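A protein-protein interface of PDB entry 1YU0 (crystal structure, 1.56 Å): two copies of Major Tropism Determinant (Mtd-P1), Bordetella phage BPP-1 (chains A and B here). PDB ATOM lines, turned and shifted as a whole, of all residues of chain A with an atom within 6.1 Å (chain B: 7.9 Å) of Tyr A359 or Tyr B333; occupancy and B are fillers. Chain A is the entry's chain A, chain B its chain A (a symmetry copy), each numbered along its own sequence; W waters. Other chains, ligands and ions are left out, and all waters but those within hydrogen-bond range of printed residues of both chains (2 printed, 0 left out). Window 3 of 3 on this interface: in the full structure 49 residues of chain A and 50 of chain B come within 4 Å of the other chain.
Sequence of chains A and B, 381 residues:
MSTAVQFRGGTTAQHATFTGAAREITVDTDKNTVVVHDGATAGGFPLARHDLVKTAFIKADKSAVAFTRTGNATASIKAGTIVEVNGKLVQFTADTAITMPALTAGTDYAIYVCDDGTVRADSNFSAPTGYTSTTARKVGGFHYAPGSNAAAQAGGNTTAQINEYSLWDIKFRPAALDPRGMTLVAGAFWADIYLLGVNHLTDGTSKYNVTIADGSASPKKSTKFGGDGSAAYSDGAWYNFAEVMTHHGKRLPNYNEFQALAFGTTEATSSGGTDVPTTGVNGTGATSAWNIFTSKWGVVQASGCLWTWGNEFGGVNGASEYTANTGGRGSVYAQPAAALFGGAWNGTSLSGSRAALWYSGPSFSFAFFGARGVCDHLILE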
ATOM      1  N   GLY A 314     -12.743   6.919  -5.719  1.00  0.00           N
ATOM      2  CA  GLY A 314     -11.766   6.248  -6.568  1.00  0.00           C
ATOM      3  C   GLY A 314     -12.068   4.760  -6.616  1.00  0.00           C
ATOM      4  O   GLY A 314     -12.994   4.285  -5.946  1.00  0.00           O
ATOM      5  N   GLY A 315     -11.310   4.028  -7.424  1.00  0.00           N
ATOM      6  CA  GLY A 315     -11.558   2.597  -7.606  1.00  0.00           C
ATOM      7  C   GLY A 315     -12.457   2.307  -8.783  1.00  0.00           C
ATOM      8  O   GLY A 315     -12.313   2.899  -9.857  1.00  0.00           O
ATOM      9  N   VAL A 316     -13.389   1.386  -8.577  1.00  0.00           N
ATOM     10  CA  VAL A 316     -14.264   0.916  -9.646  1.00  0.00           C
ATOM     11  C   VAL A 316     -15.261   1.995 -10.004  1.00  0.00           C
ATOM     12  O   VAL A 316     -15.896   2.581  -9.125  1.00  0.00           O
ATOM     13  CB  VAL A 316     -15.040  -0.325  -9.211  1.00  0.00           C
ATOM     14  CG1 VAL A 316     -15.978  -0.783 -10.321  1.00  0.00           C
ATOM     15  CG2 VAL A 316     -14.079  -1.440  -8.837  1.00  0.00           C
ATOM     16  N   ALA A 337     -16.372   4.821  -7.266  1.00  0.00           N
ATOM     17  CA  ALA A 337     -16.771   4.327  -5.960  1.00  0.00           C
ATOM     18  C   ALA A 337     -16.444   5.344  -4.868  1.00  0.00           C
ATOM     19  O   ALA A 337     -15.479   6.101  -4.970  1.00  0.00           O
ATOM     20  CB  ALA A 337     -16.069   3.043  -5.658  1.00  0.00           C
ATOM     21  N   ALA A 338     -17.233   5.307  -3.798  1.00  0.00           N
ATOM     22  CA  ALA A 338     -16.880   5.973  -2.567  1.00  0.00           C
ATOM     23  C   ALA A 338     -16.217   4.938  -1.671  1.00  0.00           C
ATOM     24  O   ALA A 338     -16.702   3.818  -1.547  1.00  0.00           O
ATOM     25  CB  ALA A 338     -18.098   6.514  -1.896  1.00  0.00           C
ATOM     26  N   ALA A 356      -9.890  -1.510   3.152  1.00  0.00           N
ATOM     27  CA  ALA A 356     -10.502  -0.517   2.273  1.00  0.00           C
ATOM     28  C   ALA A 356     -11.102  -1.178   1.046  1.00  0.00           C
ATOM     29  O   ALA A 356     -10.442  -1.945   0.354  1.00  0.00           O
ATOM     30  CB  ALA A 356      -9.484   0.521   1.860  1.00  0.00           C
ATOM     31  N   LEU A 357     -12.360  -0.866   0.793  1.00  0.00           N
ATOM     32  CA  LEU A 357     -13.128  -1.440  -0.297  1.00  0.00           C
ATOM     33  C   LEU A 357     -13.500  -0.295  -1.228  1.00  0.00           C
ATOM     34  O   LEU A 357     -14.105   0.670  -0.781  1.00  0.00           O
ATOM     35  CB  LEU A 357     -14.375  -2.135   0.266  1.00  0.00           C
ATOM     36  CG  LEU A 357     -15.440  -2.601  -0.713  1.00  0.00           C
ATOM     37  CD1 LEU A 357     -14.891  -3.633  -1.656  1.00  0.00           C
ATOM     38  CD2 LEU A 357     -16.615  -3.153   0.081  1.00  0.00           C
ATOM     39  N   TRP A 358     -13.142  -0.413  -2.509  1.00  0.00           N
ATOM     40  CA  TRP A 358     -13.397   0.642  -3.484  1.00  0.00           C
ATOM     41  C   TRP A 358     -14.230   0.142  -4.669  1.00  0.00           C
ATOM     42  O   TRP A 358     -13.960   0.452  -5.826  1.00  0.00           O
ATOM     43  CB  TRP A 358     -12.081   1.214  -3.973  1.00  0.00           C
ATOM     44  CG  TRP A 358     -11.110   1.714  -2.891  1.00  0.00           C
ATOM     45  CD1 TRP A 358     -10.236   0.964  -2.149  1.00  0.00           C
ATOM     46  CD2 TRP A 358     -10.882   3.081  -2.501  1.00  0.00           C
ATOM     47  NE1 TRP A 358      -9.493   1.775  -1.320  1.00  0.00           N
ATOM     48  CE2 TRP A 358      -9.866   3.076  -1.524  1.00  0.00           C
ATOM     49  CE3 TRP A 358     -11.438   4.305  -2.888  1.00  0.00           C
ATOM     50  CZ2 TRP A 358      -9.400   4.250  -0.933  1.00  0.00           C
ATOM     51  CZ3 TRP A 358     -10.951   5.476  -2.315  1.00  0.00           C
ATOM     52  CH2 TRP A 358      -9.950   5.438  -1.348  1.00  0.00           C
ATOM     53  N   TYR A 359     -15.279  -0.589  -4.341  1.00  0.00           N
ATOM     54  CA  TYR A 359     -16.198  -1.187  -5.306  1.00  0.00           C
ATOM     55  C   TYR A 359     -17.526  -0.443  -5.394  1.00  0.00           C
ATOM     56  O   TYR A 359     -18.150  -0.380  -6.462  1.00  0.00           O
ATOM     57  CB  TYR A 359     -16.439  -2.619  -4.831  1.00  0.00           C
ATOM     58  CG  TYR A 359     -17.621  -3.367  -5.387  1.00  0.00           C
ATOM     59  CD1 TYR A 359     -17.470  -4.197  -6.482  1.00  0.00           C
ATOM     60  CD2 TYR A 359     -18.857  -3.330  -4.751  1.00  0.00           C
ATOM     61  CE1 TYR A 359     -18.548  -4.943  -6.970  1.00  0.00           C
ATOM     62  CE2 TYR A 359     -19.941  -4.060  -5.237  1.00  0.00           C
ATOM     63  CZ  TYR A 359     -19.771  -4.860  -6.342  1.00  0.00           C
ATOM     64  OH  TYR A 359     -20.839  -5.604  -6.827  1.00  0.00           O
ATOM     65  N   SER A 360     -17.987   0.067  -4.260  1.00  0.00           N
ATOM     66  CA  SER A 360     -19.378   0.503  -4.110  1.00  0.00           C
ATOM     67  C   SER A 360     -19.595   1.931  -4.541  1.00  0.00           C
ATOM     68  O   SER A 360     -18.951   2.841  -4.036  1.00  0.00           O
ATOM     69  CB  SER A 360     -19.832   0.373  -2.652  1.00  0.00           C
ATOM     70  OG  SER A 360     -19.726  -0.968  -2.213  1.00  0.00           O
ATOM     71  N   GLY A 361     -20.517   2.145  -5.467  1.00  0.00           N
ATOM     72  CA  GLY A 361     -20.928   3.488  -5.796  1.00  0.00           C
ATOM     73  C   GLY A 361     -21.662   4.122  -4.631  1.00  0.00           C
ATOM     74  O   GLY A 361     -22.187   3.415  -3.766  1.00  0.00           O
ATOM     75  N   PHE A 364     -25.070   2.875  -3.427  1.00  0.00           N
ATOM     76  CA  PHE A 364     -25.240   1.503  -2.935  1.00  0.00           C
ATOM     77  C   PHE A 364     -25.664   1.530  -1.466  1.00  0.00           C
ATOM     78  O   PHE A 364     -25.348   2.459  -0.724  1.00  0.00           O
ATOM     79  CB  PHE A 364     -23.954   0.677  -3.069  1.00  0.00           C
ATOM     80  CG  PHE A 364     -23.554   0.315  -4.483  1.00  0.00           C
ATOM     81  CD1 PHE A 364     -23.970   1.046  -5.590  1.00  0.00           C
ATOM     82  CD2 PHE A 364     -22.671  -0.736  -4.698  1.00  0.00           C
ATOM     83  CE1 PHE A 364     -23.528   0.694  -6.883  1.00  0.00           C
ATOM     84  CE2 PHE A 364     -22.229  -1.069  -5.977  1.00  0.00           C
ATOM     85  CZ  PHE A 364     -22.663  -0.358  -7.060  1.00  0.00           C
ATOM     86  N   PHE A 366     -26.246  -1.333   1.865  1.00  0.00           N
ATOM     87  CA  PHE A 366     -26.099  -2.689   2.413  1.00  0.00           C
ATOM     88  C   PHE A 366     -26.125  -2.651   3.928  1.00  0.00           C
ATOM     89  O   PHE A 366     -25.769  -1.655   4.547  1.00  0.00           O
ATOM     90  CB  PHE A 366     -24.792  -3.337   1.954  1.00  0.00           C
ATOM     91  CG  PHE A 366     -24.799  -3.781   0.523  1.00  0.00           C
ATOM     92  CD1 PHE A 366     -25.241  -5.054   0.172  1.00  0.00           C
ATOM     93  CD2 PHE A 366     -24.394  -2.929  -0.483  1.00  0.00           C
ATOM     94  CE1 PHE A 366     -25.246  -5.461  -1.158  1.00  0.00           C
ATOM     95  CE2 PHE A 366     -24.396  -3.335  -1.815  1.00  0.00           C
ATOM     96  CZ  PHE A 366     -24.822  -4.600  -2.150  1.00  0.00           C
ATOM     97  N   PHE A 369     -22.822  -1.613   5.641  1.00  0.00           N
ATOM     98  CA  PHE A 369     -22.208  -0.296   5.393  1.00  0.00           C
ATOM     99  C   PHE A 369     -22.907   0.747   6.256  1.00  0.00           C
ATOM    100  O   PHE A 369     -24.098   0.993   6.103  1.00  0.00           O
ATOM    101  CB  PHE A 369     -22.316   0.177   3.934  1.00  0.00           C
ATOM    102  CG  PHE A 369     -21.740  -0.750   2.892  1.00  0.00           C
ATOM    103  CD1 PHE A 369     -20.843  -1.772   3.179  1.00  0.00           C
ATOM    104  CD2 PHE A 369     -22.095  -0.540   1.565  1.00  0.00           C
ATOM    105  CE1 PHE A 369     -20.335  -2.578   2.157  1.00  0.00           C
ATOM    106  CE2 PHE A 369     -21.589  -1.347   0.553  1.00  0.00           C
ATOM    107  CZ  PHE A 369     -20.741  -2.371   0.855  1.00  0.00           C
ATOM    108  N   ASN B 317      -5.869   1.358 -10.735  1.00  0.00           N
ATOM    109  CA  ASN B 317      -6.314   0.550  -9.615  1.00  0.00           C
ATOM    110  C   ASN B 317      -5.523  -0.737  -9.464  1.00  0.00           C
ATOM    111  O   ASN B 317      -5.074  -1.342 -10.453  1.00  0.00           O
ATOM    112  CB  ASN B 317      -7.791   0.182  -9.775  1.00  0.00           C
ATOM    113  CG  ASN B 317      -8.705   1.386  -9.734  1.00  0.00           C
ATOM    114  OD1 ASN B 317      -8.398   2.398  -9.117  1.00  0.00           O
ATOM    115  ND2 ASN B 317      -9.847   1.274 -10.408  1.00  0.00           N
ATOM    116  N   GLY B 318      -5.377  -1.167  -8.225  1.00  0.00           N
ATOM    117  CA  GLY B 318      -4.903  -2.512  -7.952  1.00  0.00           C
ATOM    118  C   GLY B 318      -5.996  -3.532  -8.249  1.00  0.00           C
ATOM    119  O   GLY B 318      -7.084  -3.209  -8.746  1.00  0.00           O
ATOM    120  N   ALA B 319      -5.709  -4.780  -7.912  1.00  0.00           N
ATOM    121  CA  ALA B 319      -6.583  -5.887  -8.277  1.00  0.00           C
ATOM    122  C   ALA B 319      -7.959  -5.781  -7.642  1.00  0.00           C
ATOM    123  O   ALA B 319      -8.092  -5.338  -6.496  1.00  0.00           O
ATOM    124  CB  ALA B 319      -5.943  -7.192  -7.870  1.00  0.00           C
ATOM    125  N   SER B 320      -8.977  -6.218  -8.387  1.00  0.00           N
ATOM    126  CA  SER B 320     -10.338  -6.364  -7.873  1.00  0.00           C
ATOM    127  C   SER B 320     -10.479  -7.691  -7.134  1.00  0.00           C
ATOM    128  O   SER B 320     -11.256  -8.590  -7.504  1.00  0.00           O
ATOM    129  CB  SER B 320     -11.371  -6.232  -8.997  1.00  0.00           C
ATOM    130  OG  SER B 320     -11.464  -4.880  -9.427  1.00  0.00           O
ATOM    131  N   GLU B 321      -9.703  -7.779  -6.068  1.00  0.00           N
ATOM    132  CA  GLU B 321      -9.710  -8.882  -5.139  1.00  0.00           C
ATOM    133  C   GLU B 321      -9.083  -8.375  -3.854  1.00  0.00           C
ATOM    134  O   GLU B 321      -8.231  -7.480  -3.876  1.00  0.00           O
ATOM    135  CB  GLU B 321      -8.932 -10.058  -5.689  1.00  0.00           C
ATOM    136  CG  GLU B 321      -7.448  -9.879  -5.757  1.00  0.00           C
ATOM    137  CD  GLU B 321      -6.771 -10.877  -6.684  1.00  0.00           C
ATOM    138  OE1 GLU B 321      -7.458 -11.795  -7.189  1.00  0.00           O
ATOM    139  OE2 GLU B 321      -5.549 -10.740  -6.903  1.00  0.00           O
ATOM    140  N   TYR B 322      -9.500  -8.939  -2.730  1.00  0.00           N
ATOM    141  CA  TYR B 322      -8.947  -8.511  -1.454  1.00  0.00           C
ATOM    142  C   TYR B 322      -7.465  -8.863  -1.389  1.00  0.00           C
ATOM    143  O   TYR B 322      -7.072 -10.015  -1.588  1.00  0.00           O
ATOM    144  CB  TYR B 322      -9.739  -9.108  -0.286  1.00  0.00           C
ATOM    145  CG  TYR B 322     -11.036  -8.360  -0.030  1.00  0.00           C
ATOM    146  CD1 TYR B 322     -11.025  -7.110   0.586  1.00  0.00           C
ATOM    147  CD2 TYR B 322     -12.259  -8.900  -0.396  1.00  0.00           C
ATOM    148  CE1 TYR B 322     -12.196  -6.427   0.834  1.00  0.00           C
ATOM    149  CE2 TYR B 322     -13.429  -8.210  -0.155  1.00  0.00           C
ATOM    150  CZ  TYR B 322     -13.382  -6.976   0.463  1.00  0.00           C
ATOM    151  OH  TYR B 322     -14.554  -6.288   0.722  1.00  0.00           O
ATOM    152  N   THR B 323      -6.649  -7.848  -1.123  1.00  0.00           N
ATOM    153  CA  THR B 323      -5.204  -7.959  -1.158  1.00  0.00           C
ATOM    154  C   THR B 323      -4.599  -7.458   0.160  1.00  0.00           C
ATOM    155  O   THR B 323      -4.832  -6.329   0.577  1.00  0.00           O
ATOM    156  CB  THR B 323      -4.649  -7.166  -2.337  1.00  0.00           C
ATOM    157  OG1 THR B 323      -5.344  -7.547  -3.537  1.00  0.00           O
ATOM    158  CG2 THR B 323      -3.185  -7.418  -2.494  1.00  0.00           C
ATOM    159  N   ALA B 324      -3.835  -8.322   0.825  1.00  0.00           N
ATOM    160  CA  ALA B 324      -3.263  -8.014   2.131  1.00  0.00           C
ATOM    161  C   ALA B 324      -1.889  -7.402   1.963  1.00  0.00           C
ATOM    162  O   ALA B 324      -0.860  -8.077   2.071  1.00  0.00           O
ATOM    163  CB  ALA B 324      -3.203  -9.270   2.991  1.00  0.00           C
ATOM    164  N   ASN B 325      -1.880  -6.107   1.680  1.00  0.00           N
ATOM    165  CA  ASN B 325      -0.646  -5.391   1.410  1.00  0.00           C
ATOM    166  C   ASN B 325      -0.527  -4.125   2.241  1.00  0.00           C
ATOM    167  O   ASN B 325       0.123  -3.167   1.826  1.00  0.00           O
ATOM    168  CB  ASN B 325      -0.536  -5.082  -0.092  1.00  0.00           C
ATOM    169  CG  ASN B 325      -1.703  -4.291  -0.610  1.00  0.00           C
ATOM    170  OD1 ASN B 325      -2.501  -3.793   0.172  1.00  0.00           O
ATOM    171  ND2 ASN B 325      -1.820  -4.176  -1.932  1.00  0.00           N
ATOM    172  N   SER B 331      -7.069  -5.883   4.434  1.00  0.00           N
ATOM    173  CA  SER B 331      -6.955  -6.027   2.994  1.00  0.00           C
ATOM    174  C   SER B 331      -7.704  -4.950   2.235  1.00  0.00           C
ATOM    175  O   SER B 331      -8.636  -4.330   2.757  1.00  0.00           O
ATOM    176  CB  SER B 331      -7.485  -7.402   2.574  1.00  0.00           C
ATOM    177  OG  SER B 331      -6.626  -8.428   3.064  1.00  0.00           O
ATOM    178  N   VAL B 332      -7.268  -4.738   0.990  1.00  0.00           N
ATOM    179  CA  VAL B 332      -7.862  -3.730   0.113  1.00  0.00           C
ATOM    180  C   VAL B 332      -8.378  -4.349  -1.176  1.00  0.00           C
ATOM    181  O   VAL B 332      -7.796  -5.296  -1.696  1.00  0.00           O
ATOM    182  CB  VAL B 332      -6.881  -2.595  -0.211  1.00  0.00           C
ATOM    183  CG1 VAL B 332      -6.377  -1.971   1.067  1.00  0.00           C
ATOM    184  CG2 VAL B 332      -5.697  -3.082  -1.044  1.00  0.00           C
ATOM    185  N   TYR B 333      -9.459  -3.773  -1.696  1.00  0.00           N
ATOM    186  CA  TYR B 333     -10.128  -4.260  -2.903  1.00  0.00           C
ATOM    187  C   TYR B 333     -10.252  -3.126  -3.912  1.00  0.00           C
ATOM    188  O   TYR B 333     -10.822  -2.089  -3.580  1.00  0.00           O
ATOM    189  CB  TYR B 333     -11.518  -4.822  -2.544  1.00  0.00           C
ATOM    190  CG  TYR B 333     -12.278  -5.445  -3.699  1.00  0.00           C
ATOM    191  CD1 TYR B 333     -12.412  -6.823  -3.809  1.00  0.00           C
ATOM    192  CD2 TYR B 333     -12.860  -4.646  -4.674  1.00  0.00           C
ATOM    193  CE1 TYR B 333     -13.107  -7.380  -4.888  1.00  0.00           C
ATOM    194  CE2 TYR B 333     -13.561  -5.197  -5.737  1.00  0.00           C
ATOM    195  CZ  TYR B 333     -13.671  -6.552  -5.829  1.00  0.00           C
ATOM    196  OH  TYR B 333     -14.366  -7.077  -6.901  1.00  0.00           O
ATOM    197  N   ALA B 334      -9.766  -3.358  -5.136  1.00  0.00           N
ATOM    198  CA  ALA B 334      -9.734  -2.370  -6.217  1.00  0.00           C
ATOM    199  C   ALA B 334      -9.091  -1.066  -5.775  1.00  0.00           C
ATOM    200  O   ALA B 334      -9.532   0.024  -6.144  1.00  0.00           O
ATOM    201  CB  ALA B 334     -11.119  -2.124  -6.777  1.00  0.00           C
ATOM    202  N   GLN B 335      -8.010  -1.191  -5.013  1.00  0.00           N
ATOM    203  CA  GLN B 335      -7.360  -0.033  -4.406  1.00  0.00           C
ATOM    204  C   GLN B 335      -6.843   0.953  -5.440  1.00  0.00           C
ATOM    205  O   GLN B 335      -5.958   0.607  -6.221  1.00  0.00           O
ATOM    206  CB  GLN B 335      -6.198  -0.508  -3.534  1.00  0.00           C
ATOM    207  CG  GLN B 335      -5.369   0.592  -2.888  1.00  0.00           C
ATOM    208  CD  GLN B 335      -6.169   1.453  -1.944  1.00  0.00           C
ATOM    209  OE1 GLN B 335      -6.792   0.959  -1.000  1.00  0.00           O
ATOM    210  NE2 GLN B 335      -6.180   2.765  -2.209  1.00  0.00           N
ATOM    211  N   PRO B 336      -7.360   2.198  -5.440  1.00  0.00           N
ATOM    212  CA  PRO B 336      -6.788   3.196  -6.331  1.00  0.00           C
ATOM    213  C   PRO B 336      -5.389   3.633  -5.915  1.00  0.00           C
ATOM    214  O   PRO B 336      -5.044   3.603  -4.738  1.00  0.00           O
ATOM    215  CB  PRO B 336      -7.763   4.376  -6.205  1.00  0.00           C
ATOM    216  CG  PRO B 336      -8.381   4.224  -4.873  1.00  0.00           C
ATOM    217  CD  PRO B 336      -8.503   2.735  -4.686  1.00  0.00           C
HETATM  218  O   HOH W   1     -11.547   2.781 -12.455  1.00  0.00           O
HETATM  219  O   HOH W   2      -9.333   4.936  -9.473  1.00  0.00           O
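O of Gly A315 sits at hydrogen-bond distance from ND2 of Asn B317.
N of Ala A356 lies within hydrogen-bond range of O of Ser B331 (3.1 Å).
O of Ala A356 is in hydrogen-bond range of N of Tyr B333.
N of Trp A358 sits at hydrogen-bond distance from O of Tyr B333, 3.1 Å away.
NE1 of Trp A358 lies within hydrogen-bond range of OE1 of Gln B335 (2.8 Å).
The backbone carbonyl oxygen (O) of Val A316 lies within hydrogen-bond range of the backbone NH (N) of Ala A337, 2.9 Å away.
O of Trp A358 lies within hydrogen-bond range of N of Val A316 (3.0 Å).
The backbone NH (N) of Gly B318 is in hydrogen-bond range of the backbone carbonyl oxygen (O) of Gln B335 (2.7 Å).
The backbone carbonyl oxygen of Ala B319 lies within hydrogen-bond range of the backbone NH of Ala B334, 2.9 Å away.
The backbone NH of Thr B323 sits at hydrogen-bond distance from the backbone carbonyl oxygen of Val B332.
Among the printed residues, merely in contact across the chains: Ala A356 with Val B332, Trp A358 with Pro B336, Trp A358 with Ala B334, Leu A357 with Tyr B322, Gly A315 with Ala B334, Val A316 with Ala B334, Leu A357 with Tyr B333, Gly A315 with Pro B336, Ala A356 with Gln B335, Tyr A359 with Tyr B333 and Val A316 with Asn B317.
Of chain B, only Tyr B333 comes within 4 Å of Tyr A359.
Tyr B333 touches four residues of chain A.
Of the printed residues of chain A, Pro B336 touches Gly A315 and Trp A358.
Of the printed residues of chain A, Tyr B322 touches Leu A357 (3.6 Å).
Of the printed residues of chain B, Gly A315 touches Asn B317, Ala B334 and Pro B336.
The nearest residue of chain B that does not touch Tyr A359 is Ala B334 (5.1 Å).
The nearest residue of chain A that does not touch Tyr B333 is Val A316 (4.9 Å).
The nearest printed residue of chain B that does not touch Trp A358 is Val B332 (5.2 Å).
Of the 15 printed residues of chain B, 8 touch a printed residue of chain A.
Hydrophobic or aromatic side chains of chain B within 4 Å of the printed part of chain A: Tyr B322, Val B332, Tyr B333, Ala B334 and Pro B336.
Of the 14 printed residues of chain A, 6 touch a printed residue of chain B.
Among the printed residues, 16 pairs touch across the chains.
Among the printed residues, no Asp or Glu carboxylate lies within 4 Å of a Lys or Arg side-chain nitrogen of the other chain.
No position is printed for both chains.
Of the 16 pairs that touch across the chains among the printed residues, none has its exchanged pair printed and touching as well.
Water W1 lies within hydrogen-bond range of O of Gly A315 and ND2 of Asn B317.
Water W2 bridges OD1 of Asn B317 and N of Gly A315.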
